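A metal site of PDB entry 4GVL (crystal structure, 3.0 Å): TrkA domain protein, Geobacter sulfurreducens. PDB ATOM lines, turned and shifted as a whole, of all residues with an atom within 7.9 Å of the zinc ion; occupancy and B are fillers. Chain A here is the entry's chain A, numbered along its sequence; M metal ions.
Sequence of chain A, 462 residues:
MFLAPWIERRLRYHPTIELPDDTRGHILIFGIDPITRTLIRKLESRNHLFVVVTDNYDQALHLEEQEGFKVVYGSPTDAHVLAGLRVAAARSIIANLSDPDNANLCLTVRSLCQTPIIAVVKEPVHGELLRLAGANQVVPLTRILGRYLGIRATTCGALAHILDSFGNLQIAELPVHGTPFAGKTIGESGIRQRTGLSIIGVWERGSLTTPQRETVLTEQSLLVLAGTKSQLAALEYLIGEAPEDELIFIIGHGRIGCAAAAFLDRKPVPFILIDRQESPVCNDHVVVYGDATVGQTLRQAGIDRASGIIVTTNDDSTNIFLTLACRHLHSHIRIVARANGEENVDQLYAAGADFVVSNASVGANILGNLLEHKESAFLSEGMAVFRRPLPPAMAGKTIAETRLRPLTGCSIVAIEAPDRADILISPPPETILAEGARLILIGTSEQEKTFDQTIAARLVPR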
ATOM      1  N   HIS A 253      19.194  -5.918 -21.639  1.00  0.00           N
ATOM      2  CA  HIS A 253      20.543  -5.798 -22.162  1.00  0.00           C
ATOM      3  C   HIS A 253      21.524  -6.599 -21.301  1.00  0.00           C
ATOM      4  O   HIS A 253      22.677  -6.213 -21.129  1.00  0.00           O
ATOM      5  CB  HIS A 253      20.949  -4.322 -22.308  1.00  0.00           C
ATOM      6  CG  HIS A 253      22.386  -4.116 -22.693  1.00  0.00           C
ATOM      7  ND1 HIS A 253      23.326  -3.638 -21.804  1.00  0.00           N
ATOM      8  CD2 HIS A 253      23.043  -4.345 -23.852  1.00  0.00           C
ATOM      9  CE1 HIS A 253      24.503  -3.579 -22.406  1.00  0.00           C
ATOM     10  NE2 HIS A 253      24.354  -3.991 -23.644  1.00  0.00           N
ATOM     11  N   GLY A 254      21.045  -7.717 -20.756  1.00  0.00           N
ATOM     12  CA  GLY A 254      21.943  -8.739 -20.238  1.00  0.00           C
ATOM     13  C   GLY A 254      22.660  -9.397 -21.415  1.00  0.00           C
ATOM     14  O   GLY A 254      22.649  -8.870 -22.549  1.00  0.00           O
ATOM     15  N   ARG A 255      23.252 -10.564 -21.181  1.00  0.00           N
ATOM     16  CA  ARG A 255      24.029 -11.207 -22.231  1.00  0.00           C
ATOM     17  C   ARG A 255      23.279 -11.391 -23.567  1.00  0.00           C
ATOM     18  O   ARG A 255      23.744 -10.945 -24.620  1.00  0.00           O
ATOM     19  CB  ARG A 255      24.662 -12.494 -21.713  1.00  0.00           C
ATOM     20  CG  ARG A 255      25.788 -12.208 -20.724  1.00  0.00           C
ATOM     21  CD  ARG A 255      26.585 -13.441 -20.361  1.00  0.00           C
ATOM     22  NE  ARG A 255      28.031 -13.203 -20.494  1.00  0.00           N
ATOM     23  CZ  ARG A 255      28.876 -12.994 -19.487  1.00  0.00           C
ATOM     24  NH1 ARG A 255      28.444 -12.990 -18.225  1.00  0.00           N
ATOM     25  NH2 ARG A 255      30.166 -12.803 -19.730  1.00  0.00           N
ATOM     26  N   GLY A 257      20.426 -10.028 -24.902  1.00  0.00           N
ATOM     27  CA  GLY A 257      20.123  -8.751 -25.552  1.00  0.00           C
ATOM     28  C   GLY A 257      21.371  -8.139 -26.178  1.00  0.00           C
ATOM     29  O   GLY A 257      21.387  -7.795 -27.366  1.00  0.00           O
ATOM     30  N   CYS A 258      22.430  -8.029 -25.361  1.00  0.00           N
ATOM     31  CA  CYS A 258      23.723  -7.544 -25.813  1.00  0.00           C
ATOM     32  C   CYS A 258      24.140  -8.263 -27.096  1.00  0.00           C
ATOM     33  O   CYS A 258      24.524  -7.627 -28.067  1.00  0.00           O
ATOM     34  CB  CYS A 258      24.757  -7.760 -24.706  1.00  0.00           C
ATOM     35  SG  CYS A 258      26.260  -6.750 -24.797  1.00  0.00           S
ATOM     36  N   ALA A 259      24.005  -9.591 -27.104  1.00  0.00           N
ATOM     37  CA  ALA A 259      24.348 -10.418 -28.254  1.00  0.00           C
ATOM     38  C   ALA A 259      23.516 -10.067 -29.485  1.00  0.00           C
ATOM     39  O   ALA A 259      24.057  -9.902 -30.576  1.00  0.00           O
ATOM     40  CB  ALA A 259      24.197 -11.887 -27.909  1.00  0.00           C
ATOM     41  N   ALA A 261      21.983  -7.248 -29.955  1.00  0.00           N
ATOM     42  CA  ALA A 261      22.403  -5.893 -30.296  1.00  0.00           C
ATOM     43  C   ALA A 261      23.681  -5.893 -31.127  1.00  0.00           C
ATOM     44  O   ALA A 261      23.749  -5.202 -32.137  1.00  0.00           O
ATOM     45  CB  ALA A 261      22.584  -5.068 -29.041  1.00  0.00           C
ATOM     46  N   ALA A 262      24.666  -6.676 -30.696  1.00  0.00           N
ATOM     47  CA  ALA A 262      25.922  -6.785 -31.428  1.00  0.00           C
ATOM     48  C   ALA A 262      25.677  -7.394 -32.786  1.00  0.00           C
ATOM     49  O   ALA A 262      26.316  -7.011 -33.768  1.00  0.00           O
ATOM     50  CB  ALA A 262      26.911  -7.611 -30.651  1.00  0.00           C
ATOM     51  N   PHE A 271      19.541   0.499 -33.442  1.00  0.00           N
ATOM     52  CA  PHE A 271      18.813  -0.062 -32.326  1.00  0.00           C
ATOM     53  C   PHE A 271      18.903   0.791 -31.071  1.00  0.00           C
ATOM     54  O   PHE A 271      19.746   1.687 -30.963  1.00  0.00           O
ATOM     55  CB  PHE A 271      19.308  -1.473 -32.030  1.00  0.00           C
ATOM     56  CG  PHE A 271      20.739  -1.528 -31.623  1.00  0.00           C
ATOM     57  CD1 PHE A 271      21.097  -1.501 -30.283  1.00  0.00           C
ATOM     58  CD2 PHE A 271      21.745  -1.608 -32.591  1.00  0.00           C
ATOM     59  CE1 PHE A 271      22.440  -1.557 -29.911  1.00  0.00           C
ATOM     60  CE2 PHE A 271      23.095  -1.659 -32.230  1.00  0.00           C
ATOM     61  CZ  PHE A 271      23.446  -1.636 -30.880  1.00  0.00           C
ATOM     62  N   LEU A 273      18.589   0.258 -26.670  1.00  0.00           N
ATOM     63  CA  LEU A 273      18.522  -0.720 -25.599  1.00  0.00           C
ATOM     64  C   LEU A 273      17.970  -0.099 -24.327  1.00  0.00           C
ATOM     65  O   LEU A 273      18.227   1.083 -24.034  1.00  0.00           O
ATOM     66  CB  LEU A 273      19.918  -1.268 -25.319  1.00  0.00           C
ATOM     67  CG  LEU A 273      20.580  -2.237 -26.304  1.00  0.00           C
ATOM     68  CD1 LEU A 273      22.082  -2.033 -26.348  1.00  0.00           C
ATOM     69  CD2 LEU A 273      20.258  -3.651 -25.924  1.00  0.00           C
ATOM     70  N   SER A 279      25.173  -2.525 -17.104  1.00  0.00           N
ATOM     71  CA  SER A 279      25.804  -3.788 -17.406  1.00  0.00           C
ATOM     72  C   SER A 279      27.178  -3.916 -16.777  1.00  0.00           C
ATOM     73  O   SER A 279      28.039  -3.033 -16.949  1.00  0.00           O
ATOM     74  CB  SER A 279      25.938  -3.967 -18.913  1.00  0.00           C
ATOM     75  OG  SER A 279      26.880  -4.983 -19.198  1.00  0.00           O
ATOM     76  N   VAL A 281      29.378  -5.907 -17.641  1.00  0.00           N
ATOM     77  CA  VAL A 281      30.142  -6.691 -18.606  1.00  0.00           C
ATOM     78  C   VAL A 281      30.382  -5.962 -19.923  1.00  0.00           C
ATOM     79  O   VAL A 281      31.388  -6.180 -20.591  1.00  0.00           O
ATOM     80  CB  VAL A 281      29.462  -8.078 -18.863  1.00  0.00           C
ATOM     81  CG1 VAL A 281      30.041  -8.770 -20.105  1.00  0.00           C
ATOM     82  CG2 VAL A 281      29.574  -8.987 -17.633  1.00  0.00           C
ATOM     83  N   CYS A 282      29.453  -5.092 -20.310  1.00  0.00           N
ATOM     84  CA  CYS A 282      29.491  -4.485 -21.633  1.00  0.00           C
ATOM     85  C   CYS A 282      29.747  -2.976 -21.612  1.00  0.00           C
ATOM     86  O   CYS A 282      28.931  -2.210 -21.120  1.00  0.00           O
ATOM     87  CB  CYS A 282      28.201  -4.802 -22.388  1.00  0.00           C
ATOM     88  SG  CYS A 282      27.920  -3.759 -23.815  1.00  0.00           S
ATOM     89  N   ASN A 283      30.885  -2.562 -22.178  1.00  0.00           N
ATOM     90  CA  ASN A 283      31.223  -1.140 -22.237  1.00  0.00           C
ATOM     91  C   ASN A 283      31.009  -0.511 -23.612  1.00  0.00           C
ATOM     92  O   ASN A 283      31.260   0.680 -23.805  1.00  0.00           O
ATOM     93  CB  ASN A 283      32.651  -0.902 -21.746  1.00  0.00           C
ATOM     94  CG  ASN A 283      32.723  -0.751 -20.222  1.00  0.00           C
ATOM     95  OD1 ASN A 283      33.419  -1.515 -19.547  1.00  0.00           O
ATOM     96  ND2 ASN A 283      32.004   0.241 -19.691  1.00  0.00           N
ATOM     97  N   ASP A 284      30.504  -1.298 -24.550  1.00  0.00           N
ATOM     98  CA  ASP A 284      30.415  -0.891 -25.951  1.00  0.00           C
ATOM     99  C   ASP A 284      29.064  -0.288 -26.324  1.00  0.00           C
ATOM    100  O   ASP A 284      28.926   0.250 -27.426  1.00  0.00           O
ATOM    101  CB  ASP A 284      30.729  -2.090 -26.856  1.00  0.00           C
ATOM    102  CG  ASP A 284      32.098  -2.719 -26.570  1.00  0.00           C
ATOM    103  OD1 ASP A 284      32.504  -3.628 -27.336  1.00  0.00           O
ATOM    104  OD2 ASP A 284      32.764  -2.312 -25.582  1.00  0.00           O
ATOM    105  N   HIS A 285      28.098  -0.366 -25.419  1.00  0.00           N
ATOM    106  CA  HIS A 285      26.699  -0.090 -25.753  1.00  0.00           C
ATOM    107  C   HIS A 285      26.008   0.999 -24.925  1.00  0.00           C
ATOM    108  O   HIS A 285      25.861   0.854 -23.713  1.00  0.00           O
ATOM    109  CB  HIS A 285      25.877  -1.365 -25.620  1.00  0.00           C
ATOM    110  CG  HIS A 285      25.986  -2.291 -26.789  1.00  0.00           C
ATOM    111  ND1 HIS A 285      25.791  -3.651 -26.670  1.00  0.00           N
ATOM    112  CD2 HIS A 285      26.262  -2.053 -28.093  1.00  0.00           C
ATOM    113  CE1 HIS A 285      25.943  -4.214 -27.851  1.00  0.00           C
ATOM    114  NE2 HIS A 285      26.231  -3.271 -28.735  1.00  0.00           N
ATOM    115  N   VAL A 286      25.563   2.060 -25.598  1.00  0.00           N
ATOM    116  CA  VAL A 286      24.763   3.133 -24.978  1.00  0.00           C
ATOM    117  C   VAL A 286      23.334   2.654 -24.674  1.00  0.00           C
ATOM    118  O   VAL A 286      22.620   2.158 -25.556  1.00  0.00           O
ATOM    119  CB  VAL A 286      24.730   4.406 -25.844  1.00  0.00           C
ATOM    120  CG1 VAL A 286      25.921   5.273 -25.530  1.00  0.00           C
ATOM    121  CG2 VAL A 286      24.692   4.060 -27.332  1.00  0.00           C
ATOM    122  N   VAL A 287      22.936   2.807 -23.406  1.00  0.00           N
ATOM    123  CA  VAL A 287      21.737   2.138 -22.883  1.00  0.00           C
ATOM    124  C   VAL A 287      20.833   3.121 -22.134  1.00  0.00           C
ATOM    125  O   VAL A 287      21.292   3.858 -21.264  1.00  0.00           O
ATOM    126  CB  VAL A 287      22.142   0.973 -21.951  1.00  0.00           C
ATOM    127  CG1 VAL A 287      20.992   0.504 -21.107  1.00  0.00           C
ATOM    128  CG2 VAL A 287      22.709  -0.179 -22.754  1.00  0.00           C
HETATM  129 ZN    ZN M   1      26.097  -4.498 -24.958  1.00  0.00          ZN
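The zinc ion is bound by a ring nitrogen (ND1) of His 285 (1.9 Å), a ring nitrogen (NE2) of His 253 (2.2 Å), the side-chain sulfur (SG) of Cys 258 (2.3 Å) and the side-chain sulfur (SG) of Cys 282 (2.3 Å).
Four residues have an atom within 4 Å of the zinc ion: His 253, Cys 258, Cys 282 and His 285.
The side-chain sulfur (SG) of Cys 282 sits close to the backbone NH (N) of Asp 284 (3.6 Å). The side-chain hydroxyl (OG) of Ser 279 lies within hydrogen-bond range of the backbone NH (N) of Cys 282 (2.8 Å).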
